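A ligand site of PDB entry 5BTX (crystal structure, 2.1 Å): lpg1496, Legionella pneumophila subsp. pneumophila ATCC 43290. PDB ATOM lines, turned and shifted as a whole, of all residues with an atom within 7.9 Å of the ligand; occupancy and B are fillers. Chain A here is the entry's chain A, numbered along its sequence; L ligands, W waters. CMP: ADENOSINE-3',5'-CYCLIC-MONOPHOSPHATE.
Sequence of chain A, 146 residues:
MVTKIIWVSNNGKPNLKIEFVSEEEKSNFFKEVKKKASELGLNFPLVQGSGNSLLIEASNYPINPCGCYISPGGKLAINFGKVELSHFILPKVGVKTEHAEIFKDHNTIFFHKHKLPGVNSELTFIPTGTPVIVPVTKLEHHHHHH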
ATOM      1  N   ALA A  58      22.819  -2.934   9.679  1.00  0.00           N
ATOM      2  CA  ALA A  58      22.917  -2.416  11.031  1.00  0.00           C
ATOM      3  C   ALA A  58      21.996  -1.217  11.207  1.00  0.00           C
ATOM      4  O   ALA A  58      21.755  -0.485  10.265  1.00  0.00           O
ATOM      5  CB  ALA A  58      24.388  -2.039  11.360  1.00  0.00           C
ATOM      6  N   SER A  59      21.506  -1.004  12.432  1.00  0.00           N
ATOM      7  CA  SER A  59      20.751   0.211  12.756  1.00  0.00           C
ATOM      8  C   SER A  59      21.666   1.452  12.718  1.00  0.00           C
ATOM      9  O   SER A  59      22.896   1.310  12.812  1.00  0.00           O
ATOM     10  CB  SER A  59      20.140   0.055  14.132  1.00  0.00           C
ATOM     11  OG  SER A  59      21.153  -0.108  15.114  1.00  0.00           O
ATOM     12  N   ASN A  60      21.067   2.647  12.579  1.00  0.00           N
ATOM     13  CA  ASN A  60      21.797   3.954  12.661  1.00  0.00           C
ATOM     14  C   ASN A  60      21.170   4.795  13.774  1.00  0.00           C
ATOM     15  O   ASN A  60      20.570   5.848  13.507  1.00  0.00           O
ATOM     16  CB  ASN A  60      21.760   4.710  11.324  1.00  0.00           C
ATOM     17  CG  ASN A  60      22.776   5.869  11.253  1.00  0.00           C
ATOM     18  OD1 ASN A  60      23.029   6.588  12.234  1.00  0.00           O
ATOM     19  ND2 ASN A  60      23.344   6.066  10.056  1.00  0.00           N
ATOM     20  N   TYR A  61      21.337   4.308  15.001  1.00  0.00           N
ATOM     21  CA  TYR A  61      20.729   4.898  16.192  1.00  0.00           C
ATOM     22  C   TYR A  61      21.435   6.213  16.548  1.00  0.00           C
ATOM     23  O   TYR A  61      22.644   6.323  16.374  1.00  0.00           O
ATOM     24  CB  TYR A  61      20.906   3.889  17.329  1.00  0.00           C
ATOM     25  CG  TYR A  61      20.035   4.053  18.545  1.00  0.00           C
ATOM     26  CD1 TYR A  61      18.745   3.615  18.528  1.00  0.00           C
ATOM     27  CD2 TYR A  61      20.557   4.570  19.755  1.00  0.00           C
ATOM     28  CE1 TYR A  61      17.928   3.709  19.641  1.00  0.00           C
ATOM     29  CE2 TYR A  61      19.735   4.667  20.889  1.00  0.00           C
ATOM     30  CZ  TYR A  61      18.414   4.224  20.806  1.00  0.00           C
ATOM     31  OH  TYR A  61      17.532   4.284  21.864  1.00  0.00           O
ATOM     32  N   PRO A  62      20.680   7.227  17.018  1.00  0.00           N
ATOM     33  CA  PRO A  62      19.213   7.305  17.211  1.00  0.00           C
ATOM     34  C   PRO A  62      18.436   7.800  15.985  1.00  0.00           C
ATOM     35  O   PRO A  62      17.174   7.735  15.972  1.00  0.00           O
ATOM     36  CB  PRO A  62      19.086   8.296  18.357  1.00  0.00           C
ATOM     37  CG  PRO A  62      20.218   9.247  18.131  1.00  0.00           C
ATOM     38  CD  PRO A  62      21.355   8.451  17.522  1.00  0.00           C
ATOM     39  N   ASN A  64      18.176   6.552  12.688  1.00  0.00           N
ATOM     40  CA  ASN A  64      17.397   5.380  12.238  1.00  0.00           C
ATOM     41  C   ASN A  64      17.563   4.213  13.209  1.00  0.00           C
ATOM     42  O   ASN A  64      18.587   3.536  13.169  1.00  0.00           O
ATOM     43  CB  ASN A  64      17.790   4.938  10.812  1.00  0.00           C
ATOM     44  CG  ASN A  64      16.855   3.868  10.211  1.00  0.00           C
ATOM     45  OD1 ASN A  64      15.766   3.552  10.754  1.00  0.00           O
ATOM     46  ND2 ASN A  64      17.268   3.313   9.076  1.00  0.00           N
ATOM     47  N   PRO A  65      16.579   3.983  14.108  1.00  0.00           N
ATOM     48  CA  PRO A  65      16.681   2.851  15.056  1.00  0.00           C
ATOM     49  C   PRO A  65      16.591   1.451  14.434  1.00  0.00           C
ATOM     50  O   PRO A  65      16.887   0.465  15.099  1.00  0.00           O
ATOM     51  CB  PRO A  65      15.484   3.050  15.988  1.00  0.00           C
ATOM     52  CG  PRO A  65      14.982   4.431  15.744  1.00  0.00           C
ATOM     53  CD  PRO A  65      15.396   4.820  14.361  1.00  0.00           C
ATOM     54  N   CYS A  66      16.159   1.373  13.167  1.00  0.00           N
ATOM     55  CA  CYS A  66      15.951   0.069  12.507  1.00  0.00           C
ATOM     56  C   CYS A  66      17.226  -0.658  12.093  1.00  0.00           C
ATOM     57  O   CYS A  66      18.096  -0.071  11.460  1.00  0.00           O
ATOM     58  CB  CYS A  66      15.047   0.216  11.283  1.00  0.00           C
ATOM     59  SG  CYS A  66      13.333   0.559  11.707  1.00  0.00           S
ATOM     60  N   GLY A  67      17.304  -1.938  12.448  1.00  0.00           N
ATOM     61  CA  GLY A  67      18.393  -2.818  12.011  1.00  0.00           C
ATOM     62  C   GLY A  67      19.098  -3.547  13.160  1.00  0.00           C
ATOM     63  O   GLY A  67      18.644  -3.526  14.283  1.00  0.00           O
ATOM     64  N   CYS A  68      20.219  -4.170  12.857  1.00  0.00           N
ATOM     65  CA  CYS A  68      21.012  -4.959  13.802  1.00  0.00           C
ATOM     66  C   CYS A  68      21.972  -4.158  14.623  1.00  0.00           C
ATOM     67  O   CYS A  68      22.592  -3.204  14.138  1.00  0.00           O
ATOM     68  CB  CYS A  68      21.843  -5.963  13.033  1.00  0.00           C
ATOM     69  SG  CYS A  68      20.848  -7.152  12.140  1.00  0.00           S
ATOM     70  N   TYR A  69      22.137  -4.567  15.885  1.00  0.00           N
ATOM     71  CA  TYR A  69      23.203  -4.017  16.716  1.00  0.00           C
ATOM     72  C   TYR A  69      23.671  -5.050  17.708  1.00  0.00           C
ATOM     73  O   TYR A  69      22.964  -6.016  17.955  1.00  0.00           O
ATOM     74  CB  TYR A  69      22.769  -2.716  17.403  1.00  0.00           C
ATOM     75  CG  TYR A  69      21.799  -2.860  18.561  1.00  0.00           C
ATOM     76  CD1 TYR A  69      20.460  -2.967  18.312  1.00  0.00           C
ATOM     77  CD2 TYR A  69      22.231  -2.818  19.911  1.00  0.00           C
ATOM     78  CE1 TYR A  69      19.539  -3.072  19.336  1.00  0.00           C
ATOM     79  CE2 TYR A  69      21.296  -2.924  20.957  1.00  0.00           C
ATOM     80  CZ  TYR A  69      19.948  -3.059  20.635  1.00  0.00           C
ATOM     81  OH  TYR A  69      18.962  -3.189  21.576  1.00  0.00           O
ATOM     82  N   ILE A  70      24.853  -4.840  18.289  1.00  0.00           N
ATOM     83  CA  ILE A  70      25.348  -5.692  19.360  1.00  0.00           C
ATOM     84  C   ILE A  70      24.914  -5.089  20.720  1.00  0.00           C
ATOM     85  O   ILE A  70      25.208  -3.942  21.007  1.00  0.00           O
ATOM     86  CB  ILE A  70      26.881  -5.881  19.293  1.00  0.00           C
ATOM     87  CG1 ILE A  70      27.352  -6.310  17.895  1.00  0.00           C
ATOM     88  CG2 ILE A  70      27.321  -6.933  20.309  1.00  0.00           C
ATOM     89  CD1 ILE A  70      28.854  -6.069  17.668  1.00  0.00           C
ATOM     90  N   SER A  71      24.188  -5.870  21.528  1.00  0.00           N
ATOM     91  CA  SER A  71      23.679  -5.380  22.818  1.00  0.00           C
ATOM     92  C   SER A  71      24.820  -5.384  23.833  1.00  0.00           C
ATOM     93  O   SER A  71      25.870  -5.984  23.577  1.00  0.00           O
ATOM     94  CB  SER A  71      22.464  -6.211  23.279  1.00  0.00           C
ATOM     95  OG  SER A  71      22.808  -7.571  23.450  1.00  0.00           O
ATOM     96  N   PRO A  72      24.665  -4.691  24.990  1.00  0.00           N
ATOM     97  CA  PRO A  72      25.869  -4.607  25.878  1.00  0.00           C
ATOM     98  C   PRO A  72      26.321  -5.960  26.444  1.00  0.00           C
ATOM     99  O   PRO A  72      27.408  -6.032  27.006  1.00  0.00           O
ATOM    100  CB  PRO A  72      25.423  -3.680  27.004  1.00  0.00           C
ATOM    101  CG  PRO A  72      23.936  -3.863  27.060  1.00  0.00           C
ATOM    102  CD  PRO A  72      23.469  -4.124  25.640  1.00  0.00           C
ATOM    103  N   ALA A  77      21.163  -8.155  18.245  1.00  0.00           N
ATOM    104  CA  ALA A  77      19.861  -7.617  18.536  1.00  0.00           C
ATOM    105  C   ALA A  77      19.343  -6.969  17.284  1.00  0.00           C
ATOM    106  O   ALA A  77      20.102  -6.382  16.531  1.00  0.00           O
ATOM    107  CB  ALA A  77      19.952  -6.593  19.659  1.00  0.00           C
ATOM    108  N   ILE A  78      18.038  -7.052  17.043  1.00  0.00           N
ATOM    109  CA  ILE A  78      17.491  -6.426  15.825  1.00  0.00           C
ATOM    110  C   ILE A  78      16.336  -5.535  16.243  1.00  0.00           C
ATOM    111  O   ILE A  78      15.363  -6.023  16.809  1.00  0.00           O
ATOM    112  CB  ILE A  78      17.052  -7.470  14.757  1.00  0.00           C
ATOM    113  CG1 ILE A  78      18.227  -8.378  14.388  1.00  0.00           C
ATOM    114  CG2 ILE A  78      16.480  -6.767  13.510  1.00  0.00           C
ATOM    115  CD1 ILE A  78      17.941  -9.470  13.362  1.00  0.00           C
ATOM    116  N   ASN A  79      16.487  -4.229  16.019  1.00  0.00           N
ATOM    117  CA  ASN A  79      15.396  -3.296  16.274  1.00  0.00           C
ATOM    118  C   ASN A  79      14.501  -3.215  15.019  1.00  0.00           C
ATOM    119  O   ASN A  79      15.009  -2.965  13.931  1.00  0.00           O
ATOM    120  CB  ASN A  79      15.923  -1.918  16.653  1.00  0.00           C
ATOM    121  CG  ASN A  79      14.810  -0.958  17.052  1.00  0.00           C
ATOM    122  OD1 ASN A  79      13.707  -1.029  16.529  1.00  0.00           O
ATOM    123  ND2 ASN A  79      15.106  -0.044  17.969  1.00  0.00           N
ATOM    124  N   PHE A  80      13.206  -3.460  15.179  1.00  0.00           N
ATOM    125  CA  PHE A  80      12.247  -3.434  14.051  1.00  0.00           C
ATOM    126  C   PHE A  80      11.427  -2.133  13.959  1.00  0.00           C
ATOM    127  O   PHE A  80      10.487  -2.041  13.167  1.00  0.00           O
ATOM    128  CB  PHE A  80      11.320  -4.654  14.116  1.00  0.00           C
ATOM    129  CG  PHE A  80      12.020  -5.968  13.969  1.00  0.00           C
ATOM    130  CD1 PHE A  80      12.411  -6.419  12.718  1.00  0.00           C
ATOM    131  CD2 PHE A  80      12.332  -6.753  15.075  1.00  0.00           C
ATOM    132  CE1 PHE A  80      13.053  -7.628  12.549  1.00  0.00           C
ATOM    133  CE2 PHE A  80      13.006  -7.945  14.934  1.00  0.00           C
ATOM    134  CZ  PHE A  80      13.357  -8.398  13.671  1.00  0.00           C
ATOM    135  N   GLY A  81      11.788  -1.143  14.756  1.00  0.00           N
ATOM    136  CA  GLY A  81      11.195   0.197  14.705  1.00  0.00           C
ATOM    137  C   GLY A  81       9.892   0.229  15.476  1.00  0.00           C
ATOM    138  O   GLY A  81       9.752   1.029  16.415  1.00  0.00           O
ATOM    139  N   PHE A 103       9.636  -9.496  23.378  1.00  0.00           N
ATOM    140  CA  PHE A 103       8.885  -8.918  24.477  1.00  0.00           C
ATOM    141  C   PHE A 103       7.603  -8.295  23.945  1.00  0.00           C
ATOM    142  O   PHE A 103       7.553  -7.897  22.810  1.00  0.00           O
ATOM    143  CB  PHE A 103       9.713  -7.875  25.202  1.00  0.00           C
ATOM    144  CG  PHE A 103      11.025  -8.394  25.768  1.00  0.00           C
ATOM    145  CD1 PHE A 103      12.167  -8.478  24.975  1.00  0.00           C
ATOM    146  CD2 PHE A 103      11.121  -8.758  27.083  1.00  0.00           C
ATOM    147  CE1 PHE A 103      13.367  -8.943  25.501  1.00  0.00           C
ATOM    148  CE2 PHE A 103      12.317  -9.214  27.612  1.00  0.00           C
ATOM    149  CZ  PHE A 103      13.421  -9.318  26.832  1.00  0.00           C
ATOM    150  N   HIS A 106       7.546  -4.582  22.815  1.00  0.00           N
ATOM    151  CA  HIS A 106       8.883  -4.188  22.368  1.00  0.00           C
ATOM    152  C   HIS A 106       8.968  -4.238  20.845  1.00  0.00           C
ATOM    153  O   HIS A 106       8.175  -4.937  20.155  1.00  0.00           O
ATOM    154  CB  HIS A 106       9.960  -5.061  23.023  1.00  0.00           C
ATOM    155  CG  HIS A 106      11.243  -4.335  23.351  1.00  0.00           C
ATOM    156  ND1 HIS A 106      11.808  -3.383  22.527  1.00  0.00           N
ATOM    157  CD2 HIS A 106      12.075  -4.450  24.404  1.00  0.00           C
ATOM    158  CE1 HIS A 106      12.935  -2.952  23.050  1.00  0.00           C
ATOM    159  NE2 HIS A 106      13.128  -3.583  24.190  1.00  0.00           N
ATOM    160  N   ASN A 107       9.926  -3.491  20.296  1.00  0.00           N
ATOM    161  CA  ASN A 107      10.211  -3.487  18.881  1.00  0.00           C
ATOM    162  C   ASN A 107      11.565  -4.116  18.553  1.00  0.00           C
ATOM    163  O   ASN A 107      11.954  -4.171  17.375  1.00  0.00           O
ATOM    164  CB  ASN A 107      10.191  -2.050  18.389  1.00  0.00           C
ATOM    165  CG  ASN A 107      11.230  -1.191  19.053  1.00  0.00           C
ATOM    166  OD1 ASN A 107      11.969  -1.650  19.953  1.00  0.00           O
ATOM    167  ND2 ASN A 107      11.319   0.050  18.618  1.00  0.00           N
ATOM    168  N   THR A 108      12.261  -4.577  19.587  1.00  0.00           N
ATOM    169  CA  THR A 108      13.624  -5.117  19.466  1.00  0.00           C
ATOM    170  C   THR A 108      13.709  -6.514  20.068  1.00  0.00           C
ATOM    171  O   THR A 108      13.293  -6.735  21.189  1.00  0.00           O
ATOM    172  CB  THR A 108      14.679  -4.215  20.197  1.00  0.00           C
ATOM    173  OG1 THR A 108      14.590  -2.860  19.729  1.00  0.00           O
ATOM    174  CG2 THR A 108      16.067  -4.735  20.010  1.00  0.00           C
ATOM    175  N   ILE A 109      14.276  -7.451  19.300  1.00  0.00           N
ATOM    176  CA  ILE A 109      14.520  -8.828  19.798  1.00  0.00           C
ATOM    177  C   ILE A 109      16.014  -9.017  20.055  1.00  0.00           C
ATOM    178  O   ILE A 109      16.850  -8.290  19.506  1.00  0.00           O
ATOM    179  CB  ILE A 109      14.013  -9.929  18.825  1.00  0.00           C
ATOM    180  CG1 ILE A 109      14.884  -9.982  17.539  1.00  0.00           C
ATOM    181  CG2 ILE A 109      12.541  -9.705  18.486  1.00  0.00           C
ATOM    182  CD1 ILE A 109      14.846 -11.303  16.807  1.00  0.00           C
ATOM    183  N   PHE A 110      16.325 -10.020  20.872  1.00  0.00           N
ATOM    184  CA  PHE A 110      17.710 -10.324  21.277  1.00  0.00           C
ATOM    185  C   PHE A 110      18.002 -11.809  21.114  1.00  0.00           C
ATOM    186  O   PHE A 110      17.454 -12.629  21.854  1.00  0.00           O
ATOM    187  CB  PHE A 110      17.867  -9.953  22.753  1.00  0.00           C
ATOM    188  CG  PHE A 110      17.756  -8.479  23.025  1.00  0.00           C
ATOM    189  CD1 PHE A 110      18.880  -7.622  22.873  1.00  0.00           C
ATOM    190  CD2 PHE A 110      16.523  -7.916  23.367  1.00  0.00           C
ATOM    191  CE1 PHE A 110      18.734  -6.255  23.078  1.00  0.00           C
ATOM    192  CE2 PHE A 110      16.404  -6.550  23.615  1.00  0.00           C
ATOM    193  CZ  PHE A 110      17.494  -5.717  23.455  1.00  0.00           C
HETATM  194  P   CMP L   1      16.479  -2.303  25.301  1.00  0.00           P
HETATM  195  O1P CMP L   1      15.393  -3.271  25.691  1.00  0.00           O
HETATM  196  O2P CMP L   1      17.922  -2.609  25.686  1.00  0.00           O
HETATM  197  O5' CMP L   1      16.114  -0.835  25.834  1.00  0.00           O
HETATM  198  C5' CMP L   1      16.728   0.320  25.234  1.00  0.00           C
HETATM  199  C4' CMP L   1      16.432   0.234  23.738  1.00  0.00           C
HETATM  200  O4' CMP L   1      17.005   1.230  22.897  1.00  0.00           O
HETATM  201  C3' CMP L   1      17.003  -1.028  23.120  1.00  0.00           C
HETATM  202  O3' CMP L   1      16.390  -2.178  23.701  1.00  0.00           O
HETATM  203  C2' CMP L   1      16.820  -0.767  21.643  1.00  0.00           C
HETATM  204  O2' CMP L   1      15.447  -0.830  21.238  1.00  0.00           O
HETATM  205  C1' CMP L   1      17.188   0.694  21.592  1.00  0.00           C
HETATM  206  N9  CMP L   1      18.585   0.768  21.130  1.00  0.00           N
HETATM  207  C8  CMP L   1      19.679   1.038  21.915  1.00  0.00           C
HETATM  208  N7  CMP L   1      20.793   1.004  21.179  1.00  0.00           N
HETATM  209  C5  CMP L   1      20.423   0.686  19.901  1.00  0.00           C
HETATM  210  C6  CMP L   1      21.112   0.490  18.605  1.00  0.00           C
HETATM  211  N6  CMP L   1      22.491   0.609  18.493  1.00  0.00           N
HETATM  212  N1  CMP L   1      20.339   0.203  17.543  1.00  0.00           N
HETATM  213  C2  CMP L   1      19.004   0.074  17.601  1.00  0.00           C
HETATM  214  N3  CMP L   1      18.313   0.224  18.746  1.00  0.00           N
HETATM  215  C4  CMP L   1      18.970   0.525  19.893  1.00  0.00           C
HETATM  216  O   HOH W   1      23.582   1.762  15.759  1.00  0.00           O
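OG1 of Thr 108 sits at hydrogen-bond distance from O2' of the ligand (2.7 Å).
An oxygen (O4') of the ligand is in hydrogen-bond range of the side-chain hydroxyl (OH) of Tyr 61 (3.3 Å).
A nitrogen (N1) of the ligand sits at hydrogen-bond distance from the side-chain hydroxyl (OG) of Ser 59 (2.6 Å).
The side-chain hydroxyl (OH) of Tyr 69 sits close to an oxygen (O3') of the ligand (3.5 Å).
NE2 of His 106 lies within hydrogen-bond range of O1P of the ligand (2.7 Å).
The side-chain amide nitrogen of Asn 79 sits at hydrogen-bond distance from a nitrogen (N3) of the ligand, at 3.3 Å.
Residues that only touch the ligand: Pro 65 (3.3 Å), Phe 110 (3.7 Å) and Asn 107 (3.8 Å).
Hydrophobic or aromatic side chains within 4 Å of the ligand: Tyr 61, Tyr 69, His 106 and Phe 110.
Nine residues have an atom within 4 Å of the ligand: Ser 59, Tyr 61, Pro 65, Tyr 69, Asn 79, His 106, Asn 107, Thr 108 and Phe 110.
ND1 of His 106 sits at hydrogen-bond distance from OD1 of Asn 107, 3.1 Å away.
The side-chain amide nitrogen of Asn 107 is in hydrogen-bond range of the backbone carbonyl oxygen of Gly 81, at 2.9 Å.
The backbone NH (N) of Tyr 69 lies within hydrogen-bond range of the backbone carbonyl oxygen (O) of Ala 77 (2.8 Å).
The backbone NH (N) of Asn 79 is in hydrogen-bond range of the backbone carbonyl oxygen (O) of Gly 67 (2.9 Å).
The side-chain amide oxygen (OD1) of Asn 79 sits at hydrogen-bond distance from the backbone NH (N) of Gly 81, at 2.6 Å.
A ring nitrogen (ND1) of His 106 is in hydrogen-bond range of the backbone NH of Thr 108 (3.2 Å).
ND2 of Asn 79 sits close to O of Pro 65 (3.4 Å).
OG1 of Thr 108 sits at hydrogen-bond distance from OD1 of Asn 107 (2.9 Å).
Water W1 lies within hydrogen-bond range of the backbone carbonyl oxygen of Ser 59 (3.1 Å), a nitrogen (N6) of the ligand (3.2 Å) and the backbone NH of Tyr 61 (3.5 Å).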
